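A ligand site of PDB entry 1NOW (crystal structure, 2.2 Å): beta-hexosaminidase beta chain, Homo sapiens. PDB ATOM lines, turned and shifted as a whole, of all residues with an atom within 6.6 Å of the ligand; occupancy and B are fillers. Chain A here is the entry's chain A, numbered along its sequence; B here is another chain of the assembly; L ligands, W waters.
Water W1 lies within hydrogen-bond range of O3 of the ligand (2.7 Å) and OE1 of Glu 306 (2.8 Å).
His 245 touches the ligand (CE1 to O2, 3.9 Å). Trp 356 touches the ligand. Trp 375 touches the ligand. Trp 440 touches the ligand. Tyr 407 of chain B touches the ligand (OH to C5, 3.8 Å). Hydrophobic or aromatic side chains that line the ligand: His 245, Trp 356, Trp 375, Tyr 401 and Trp 440. Within 4 Å of the ligand: Arg 162, His 245, Asp 305, Glu 306, Trp 356, Trp 375, Tyr 401, Asp 403, Trp 440, Glu 442 and Tyr 407 of chain B. The nearest printed residue that does not touch the ligand is Leu 404 (4.1 Å).
An oxygen (O4) of the ligand is in hydrogen-bond range of the side-chain carboxylate of Asp 403 (2.7 Å). The guanidinium group (NH2) of Arg 162 lies within hydrogen-bond range of an oxygen (O2) of the ligand (3.0 Å). The side-chain carboxylate of Glu 306 lies within salt-bridge range of a nitrogen (N1) of the ligand (2.8 Å). OD2 of Asp 305 lies within hydrogen-bond range of N2 of the ligand, at 2.8 Å. OH of Tyr 401 sits at hydrogen-bond distance from O1 of the ligand (2.7 Å). The side-chain carboxylate (OE2) of Glu 442 is in hydrogen-bond range of an oxygen (O3) of the ligand, at 2.8 Å.
The indole nitrogen (NE1) of Trp 356 sits at hydrogen-bond distance from the side-chain carboxylate (OE2) of Glu 239 (2.8 Å). OD1 of Asp 191 is in hydrogen-bond range of ND1 of His 245, 2.8 Å away. The indole nitrogen (NE1) of Trp 440 sits close to the side-chain hydroxyl (OH) of Tyr 401 (3.4 Å). The side-chain carboxylate (OE2) of Glu 358 lies within hydrogen-bond range of the backbone NH (N) of Glu 306 (3.0 Å). The side-chain carboxylate of Glu 442 lies within salt-bridge range of the guanidinium group of Arg 162. NE2 of His 245 is in hydrogen-bond range of OE1 of Glu 306 (2.7 Å). The side-chain carboxylate of Asp 305 sits at hydrogen-bond distance from a ring nitrogen (NE2) of His 245 (2.9 Å). OD2 of Asp 159 lies within salt-bridge range of NH1 of Arg 162, 2.9 Å away.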
ATOM      1  N   LEU A 157      28.173   2.900  14.184  1.00  0.00           N
ATOM      2  CA  LEU A 157      26.865   2.319  13.940  1.00  0.00           C
ATOM      3  C   LEU A 157      26.252   1.926  15.257  1.00  0.00           C
ATOM      4  O   LEU A 157      26.864   1.208  16.036  1.00  0.00           O
ATOM      5  CB  LEU A 157      26.915   1.088  13.046  1.00  0.00           C
ATOM      6  CG  LEU A 157      25.584   0.385  12.750  1.00  0.00           C
ATOM      7  CD1 LEU A 157      25.602  -0.150  11.342  1.00  0.00           C
ATOM      8  CD2 LEU A 157      25.311  -0.780  13.681  1.00  0.00           C
ATOM      9  N   ASP A 159      22.474   0.354  16.838  1.00  0.00           N
ATOM     10  CA  ASP A 159      21.364  -0.512  16.448  1.00  0.00           C
ATOM     11  C   ASP A 159      20.264  -0.314  17.479  1.00  0.00           C
ATOM     12  O   ASP A 159      20.386  -0.808  18.599  1.00  0.00           O
ATOM     13  CB  ASP A 159      21.876  -1.960  16.426  1.00  0.00           C
ATOM     14  CG  ASP A 159      20.781  -3.019  16.144  1.00  0.00           C
ATOM     15  OD1 ASP A 159      19.563  -2.749  16.080  1.00  0.00           O
ATOM     16  OD2 ASP A 159      21.101  -4.222  16.003  1.00  0.00           O
ATOM     17  N   ARG A 162      17.347  -4.154  17.677  1.00  0.00           N
ATOM     18  CA  ARG A 162      17.616  -5.349  18.492  1.00  0.00           C
ATOM     19  C   ARG A 162      17.347  -5.032  19.969  1.00  0.00           C
ATOM     20  O   ARG A 162      16.851  -5.868  20.719  1.00  0.00           O
ATOM     21  CB  ARG A 162      19.011  -5.883  18.245  1.00  0.00           C
ATOM     22  CG  ARG A 162      19.152  -6.753  16.972  1.00  0.00           C
ATOM     23  CD  ARG A 162      18.543  -6.167  15.689  1.00  0.00           C
ATOM     24  NE  ARG A 162      18.768  -7.060  14.557  1.00  0.00           N
ATOM     25  CZ  ARG A 162      19.869  -7.115  13.793  1.00  0.00           C
ATOM     26  NH1 ARG A 162      20.917  -6.308  13.987  1.00  0.00           N
ATOM     27  NH2 ARG A 162      19.919  -8.002  12.803  1.00  0.00           N
ATOM     28  N   HIS A 188      21.171   2.560  12.632  1.00  0.00           N
ATOM     29  CA  HIS A 188      20.465   1.375  12.159  1.00  0.00           C
ATOM     30  C   HIS A 188      19.187   1.329  12.985  1.00  0.00           C
ATOM     31  O   HIS A 188      19.107   0.659  14.008  1.00  0.00           O
ATOM     32  CB  HIS A 188      21.330   0.121  12.316  1.00  0.00           C
ATOM     33  CG  HIS A 188      20.759  -1.078  11.629  1.00  0.00           C
ATOM     34  ND1 HIS A 188      21.009  -1.379  10.314  1.00  0.00           N
ATOM     35  CD2 HIS A 188      19.922  -2.050  12.089  1.00  0.00           C
ATOM     36  CE1 HIS A 188      20.373  -2.488   9.982  1.00  0.00           C
ATOM     37  NE2 HIS A 188      19.723  -2.921  11.050  1.00  0.00           N
ATOM     38  N   ASP A 191      14.840  -2.970  12.254  1.00  0.00           N
ATOM     39  CA  ASP A 191      15.331  -4.298  11.852  1.00  0.00           C
ATOM     40  C   ASP A 191      14.198  -5.299  12.108  1.00  0.00           C
ATOM     41  O   ASP A 191      13.055  -4.873  12.292  1.00  0.00           O
ATOM     42  CB  ASP A 191      16.637  -4.688  12.583  1.00  0.00           C
ATOM     43  CG  ASP A 191      17.529  -5.568  11.710  1.00  0.00           C
ATOM     44  OD1 ASP A 191      17.242  -6.788  11.644  1.00  0.00           O
ATOM     45  OD2 ASP A 191      18.456  -5.125  11.002  1.00  0.00           O
ATOM     46  N   GLU A 239      19.635   4.348   8.412  1.00  0.00           N
ATOM     47  CA  GLU A 239      19.540   3.106   7.663  1.00  0.00           C
ATOM     48  C   GLU A 239      18.160   2.515   7.885  1.00  0.00           C
ATOM     49  O   GLU A 239      17.768   2.290   9.018  1.00  0.00           O
ATOM     50  CB  GLU A 239      20.586   2.048   8.041  1.00  0.00           C
ATOM     51  CG  GLU A 239      20.496   0.824   7.133  1.00  0.00           C
ATOM     52  CD  GLU A 239      21.435  -0.298   7.506  1.00  0.00           C
ATOM     53  OE1 GLU A 239      22.320  -0.066   8.370  1.00  0.00           O
ATOM     54  OE2 GLU A 239      21.271  -1.431   6.962  1.00  0.00           O
ATOM     55  N   ASP A 241      16.883  -0.678   6.478  1.00  0.00           N
ATOM     56  CA  ASP A 241      17.316  -1.872   5.786  1.00  0.00           C
ATOM     57  C   ASP A 241      16.159  -2.642   5.128  1.00  0.00           C
ATOM     58  O   ASP A 241      15.162  -2.947   5.795  1.00  0.00           O
ATOM     59  CB  ASP A 241      18.016  -2.734   6.842  1.00  0.00           C
ATOM     60  CG  ASP A 241      18.824  -3.843   6.278  1.00  0.00           C
ATOM     61  OD1 ASP A 241      18.779  -4.151   5.058  1.00  0.00           O
ATOM     62  OD2 ASP A 241      19.554  -4.484   7.045  1.00  0.00           O
ATOM     63  N   HIS A 245      15.795  -8.194   6.763  1.00  0.00           N
ATOM     64  CA  HIS A 245      15.795  -7.468   8.034  1.00  0.00           C
ATOM     65  C   HIS A 245      14.542  -6.620   8.234  1.00  0.00           C
ATOM     66  O   HIS A 245      14.611  -5.601   8.906  1.00  0.00           O
ATOM     67  CB  HIS A 245      17.099  -6.662   8.246  1.00  0.00           C
ATOM     68  CG  HIS A 245      18.274  -7.543   8.513  1.00  0.00           C
ATOM     69  ND1 HIS A 245      18.350  -8.361   9.619  1.00  0.00           N
ATOM     70  CD2 HIS A 245      19.374  -7.800   7.779  1.00  0.00           C
ATOM     71  CE1 HIS A 245      19.473  -9.060   9.570  1.00  0.00           C
ATOM     72  NE2 HIS A 245      20.115  -8.732   8.454  1.00  0.00           N
ATOM     73  N   ASP A 305      21.705  -6.274   3.127  1.00  0.00           N
ATOM     74  CA  ASP A 305      22.484  -7.408   3.642  1.00  0.00           C
ATOM     75  C   ASP A 305      21.647  -8.646   3.949  1.00  0.00           C
ATOM     76  O   ASP A 305      20.445  -8.548   4.200  1.00  0.00           O
ATOM     77  CB  ASP A 305      23.214  -7.012   4.934  1.00  0.00           C
ATOM     78  CG  ASP A 305      22.256  -6.625   6.033  1.00  0.00           C
ATOM     79  OD1 ASP A 305      21.445  -5.719   5.776  1.00  0.00           O
ATOM     80  OD2 ASP A 305      22.227  -7.160   7.151  1.00  0.00           O
ATOM     81  N   GLU A 306      22.306  -9.804   3.883  1.00  0.00           N
ATOM     82  CA  GLU A 306      21.762 -11.098   4.324  1.00  0.00           C
ATOM     83  C   GLU A 306      20.341 -11.451   3.867  1.00  0.00           C
ATOM     84  O   GLU A 306      19.541 -11.939   4.666  1.00  0.00           O
ATOM     85  CB  GLU A 306      21.812 -11.172   5.870  1.00  0.00           C
ATOM     86  CG  GLU A 306      23.208 -10.986   6.460  1.00  0.00           C
ATOM     87  CD  GLU A 306      23.228 -10.831   7.991  1.00  0.00           C
ATOM     88  OE1 GLU A 306      22.202 -10.505   8.629  1.00  0.00           O
ATOM     89  OE2 GLU A 306      24.314 -11.022   8.555  1.00  0.00           O
ATOM     90  N   TRP A 356      25.078  -2.171   1.761  1.00  0.00           N
ATOM     91  CA  TRP A 356      25.990  -3.215   2.259  1.00  0.00           C
ATOM     92  C   TRP A 356      26.489  -3.991   1.037  1.00  0.00           C
ATOM     93  O   TRP A 356      25.807  -4.045   0.003  1.00  0.00           O
ATOM     94  CB  TRP A 356      25.318  -4.195   3.234  1.00  0.00           C
ATOM     95  CG  TRP A 356      24.875  -3.574   4.493  1.00  0.00           C
ATOM     96  CD1 TRP A 356      23.604  -3.431   4.905  1.00  0.00           C
ATOM     97  CD2 TRP A 356      25.695  -3.007   5.520  1.00  0.00           C
ATOM     98  NE1 TRP A 356      23.554  -2.792   6.124  1.00  0.00           N
ATOM     99  CE2 TRP A 356      24.840  -2.520   6.523  1.00  0.00           C
ATOM    100  CE3 TRP A 356      27.066  -2.870   5.696  1.00  0.00           C
ATOM    101  CZ2 TRP A 356      25.310  -1.929   7.677  1.00  0.00           C
ATOM    102  CZ3 TRP A 356      27.530  -2.278   6.837  1.00  0.00           C
ATOM    103  CH2 TRP A 356      26.658  -1.811   7.814  1.00  0.00           C
ATOM    104  N   GLU A 358      26.655  -6.955  -0.188  1.00  0.00           N
ATOM    105  CA  GLU A 358      25.907  -8.020  -0.838  1.00  0.00           C
ATOM    106  C   GLU A 358      25.240  -7.544  -2.126  1.00  0.00           C
ATOM    107  O   GLU A 358      25.190  -8.282  -3.099  1.00  0.00           O
ATOM    108  CB  GLU A 358      24.841  -8.624   0.086  1.00  0.00           C
ATOM    109  CG  GLU A 358      25.382  -9.498   1.193  1.00  0.00           C
ATOM    110  CD  GLU A 358      25.564  -8.757   2.497  1.00  0.00           C
ATOM    111  OE1 GLU A 358      26.042  -7.603   2.491  1.00  0.00           O
ATOM    112  OE2 GLU A 358      25.222  -9.316   3.556  1.00  0.00           O
ATOM    113  N   TRP A 375      31.593  -4.945   4.878  1.00  0.00           N
ATOM    114  CA  TRP A 375      31.464  -5.429   6.253  1.00  0.00           C
ATOM    115  C   TRP A 375      31.850  -6.883   6.514  1.00  0.00           C
ATOM    116  O   TRP A 375      32.061  -7.247   7.669  1.00  0.00           O
ATOM    117  CB  TRP A 375      30.031  -5.238   6.739  1.00  0.00           C
ATOM    118  CG  TRP A 375      29.026  -6.262   6.222  1.00  0.00           C
ATOM    119  CD1 TRP A 375      28.325  -6.190   5.058  1.00  0.00           C
ATOM    120  CD2 TRP A 375      28.591  -7.470   6.875  1.00  0.00           C
ATOM    121  NE1 TRP A 375      27.504  -7.290   4.934  1.00  0.00           N
ATOM    122  CE2 TRP A 375      27.645  -8.090   6.041  1.00  0.00           C
ATOM    123  CE3 TRP A 375      28.926  -8.101   8.081  1.00  0.00           C
ATOM    124  CZ2 TRP A 375      27.035  -9.294   6.365  1.00  0.00           C
ATOM    125  CZ3 TRP A 375      28.311  -9.304   8.392  1.00  0.00           C
ATOM    126  CH2 TRP A 375      27.382  -9.887   7.540  1.00  0.00           C
ATOM    127  N   TYR A 401      33.955  -4.680  13.894  1.00  0.00           N
ATOM    128  CA  TYR A 401      32.657  -5.103  14.417  1.00  0.00           C
ATOM    129  C   TYR A 401      32.848  -5.184  15.932  1.00  0.00           C
ATOM    130  O   TYR A 401      33.298  -6.198  16.457  1.00  0.00           O
ATOM    131  CB  TYR A 401      32.203  -6.409  13.750  1.00  0.00           C
ATOM    132  CG  TYR A 401      31.266  -6.153  12.598  1.00  0.00           C
ATOM    133  CD1 TYR A 401      31.496  -5.103  11.700  1.00  0.00           C
ATOM    134  CD2 TYR A 401      30.129  -6.911  12.420  1.00  0.00           C
ATOM    135  CE1 TYR A 401      30.630  -4.840  10.681  1.00  0.00           C
ATOM    136  CE2 TYR A 401      29.277  -6.665  11.402  1.00  0.00           C
ATOM    137  CZ  TYR A 401      29.519  -5.622  10.521  1.00  0.00           C
ATOM    138  OH  TYR A 401      28.619  -5.340   9.533  1.00  0.00           O
ATOM    139  N   ASP A 403      30.658  -5.242  18.279  1.00  0.00           N
ATOM    140  CA  ASP A 403      29.791  -6.194  18.965  1.00  0.00           C
ATOM    141  C   ASP A 403      30.478  -7.561  19.191  1.00  0.00           C
ATOM    142  O   ASP A 403      30.148  -8.266  20.160  1.00  0.00           O
ATOM    143  CB  ASP A 403      28.474  -6.342  18.205  1.00  0.00           C
ATOM    144  CG  ASP A 403      28.639  -6.907  16.814  1.00  0.00           C
ATOM    145  OD1 ASP A 403      29.540  -6.451  16.049  1.00  0.00           O
ATOM    146  OD2 ASP A 403      27.871  -7.802  16.390  1.00  0.00           O
ATOM    147  N   LEU A 404      31.459  -7.904  18.348  1.00  0.00           N
ATOM    148  CA  LEU A 404      32.213  -9.143  18.480  1.00  0.00           C
ATOM    149  C   LEU A 404      33.336  -8.970  19.507  1.00  0.00           C
ATOM    150  O   LEU A 404      34.507  -8.767  19.165  1.00  0.00           O
ATOM    151  CB  LEU A 404      32.770  -9.599  17.114  1.00  0.00           C
ATOM    152  CG  LEU A 404      31.783  -9.701  15.931  1.00  0.00           C
ATOM    153  CD1 LEU A 404      32.501 -10.124  14.629  1.00  0.00           C
ATOM    154  CD2 LEU A 404      30.648 -10.645  16.202  1.00  0.00           C
ATOM    155  N   TRP A 440      26.469  -3.644  16.671  1.00  0.00           N
ATOM    156  CA  TRP A 440      25.179  -4.312  16.478  1.00  0.00           C
ATOM    157  C   TRP A 440      24.583  -4.629  17.836  1.00  0.00           C
ATOM    158  O   TRP A 440      25.304  -4.785  18.831  1.00  0.00           O
ATOM    159  CB  TRP A 440      25.320  -5.550  15.602  1.00  0.00           C
ATOM    160  CG  TRP A 440      25.766  -5.160  14.248  1.00  0.00           C
ATOM    161  CD1 TRP A 440      27.042  -5.167  13.774  1.00  0.00           C
ATOM    162  CD2 TRP A 440      24.956  -4.593  13.222  1.00  0.00           C
ATOM    163  NE1 TRP A 440      27.063  -4.665  12.487  1.00  0.00           N
ATOM    164  CE2 TRP A 440      25.797  -4.312  12.117  1.00  0.00           C
ATOM    165  CE3 TRP A 440      23.590  -4.323  13.099  1.00  0.00           C
ATOM    166  CZ2 TRP A 440      25.316  -3.793  10.915  1.00  0.00           C
ATOM    167  CZ3 TRP A 440      23.108  -3.816  11.904  1.00  0.00           C
ATOM    168  CH2 TRP A 440      23.965  -3.544  10.830  1.00  0.00           C
ATOM    169  N   GLY A 441      23.258  -4.702  17.863  1.00  0.00           N
ATOM    170  CA  GLY A 441      22.502  -4.683  19.093  1.00  0.00           C
ATOM    171  C   GLY A 441      21.964  -5.940  19.710  1.00  0.00           C
ATOM    172  O   GLY A 441      21.268  -5.831  20.715  1.00  0.00           O
ATOM    173  N   GLU A 442      22.274  -7.111  19.159  1.00  0.00           N
ATOM    174  CA  GLU A 442      21.732  -8.367  19.717  1.00  0.00           C
ATOM    175  C   GLU A 442      21.985  -8.502  21.202  1.00  0.00           C
ATOM    176  O   GLU A 442      21.111  -8.937  21.937  1.00  0.00           O
ATOM    177  CB  GLU A 442      22.332  -9.594  19.012  1.00  0.00           C
ATOM    178  CG  GLU A 442      21.777  -9.896  17.627  1.00  0.00           C
ATOM    179  CD  GLU A 442      22.378  -9.061  16.503  1.00  0.00           C
ATOM    180  OE1 GLU A 442      23.305  -8.253  16.735  1.00  0.00           O
ATOM    181  OE2 GLU A 442      21.919  -9.218  15.365  1.00  0.00           O
ATOM    182  N   TYR B 407      31.836 -13.553  22.284  1.00  0.00           N
ATOM    183  CA  TYR B 407      30.640 -13.143  21.582  1.00  0.00           C
ATOM    184  C   TYR B 407      29.477 -14.105  21.801  1.00  0.00           C
ATOM    185  O   TYR B 407      29.632 -15.314  21.706  1.00  0.00           O
ATOM    186  CB  TYR B 407      30.898 -13.044  20.083  1.00  0.00           C
ATOM    187  CG  TYR B 407      29.677 -12.592  19.319  1.00  0.00           C
ATOM    188  CD1 TYR B 407      29.201 -11.296  19.453  1.00  0.00           C
ATOM    189  CD2 TYR B 407      28.980 -13.464  18.467  1.00  0.00           C
ATOM    190  CE1 TYR B 407      28.087 -10.865  18.776  1.00  0.00           C
ATOM    191  CE2 TYR B 407      27.848 -13.032  17.775  1.00  0.00           C
ATOM    192  CZ  TYR B 407      27.405 -11.721  17.929  1.00  0.00           C
ATOM    193  OH  TYR B 407      26.291 -11.256  17.255  1.00  0.00           O
HETATM  194  N1  LIG L   1      25.385  -9.121  10.352  1.00  0.00           N
HETATM  195  C1  LIG L   1      24.230  -8.267  10.219  1.00  0.00           C
HETATM  196  C2  LIG L   1      23.798  -7.414  11.433  1.00  0.00           C
HETATM  197  C3  LIG L   1      24.092  -8.070  12.796  1.00  0.00           C
HETATM  198  C4  LIG L   1      25.534  -8.545  12.789  1.00  0.00           C
HETATM  199  C5  LIG L   1      26.026  -9.145  14.084  1.00  0.00           C
HETATM  200  C6  LIG L   1      25.365  -6.645   8.804  1.00  0.00           C
HETATM  201  C7  LIG L   1      25.440  -5.614   7.719  1.00  0.00           C
HETATM  202  C8  LIG L   1      25.788  -9.563  11.684  1.00  0.00           C
HETATM  203  N2  LIG L   1      24.291  -7.472   9.020  1.00  0.00           N
HETATM  204  O1  LIG L   1      26.336  -6.707   9.556  1.00  0.00           O
HETATM  205  O2  LIG L   1      22.412  -7.142  11.341  1.00  0.00           O
HETATM  206  O3  LIG L   1      23.233  -9.190  12.942  1.00  0.00           O
HETATM  207  O4  LIG L   1      27.447  -9.206  14.111  1.00  0.00           O
HETATM  208  O   HOH W   1      21.787 -10.827  11.356  1.00  0.00           O
HETATM  209  O   HOH W   2      21.085  -5.745   9.581  1.00  0.00           O
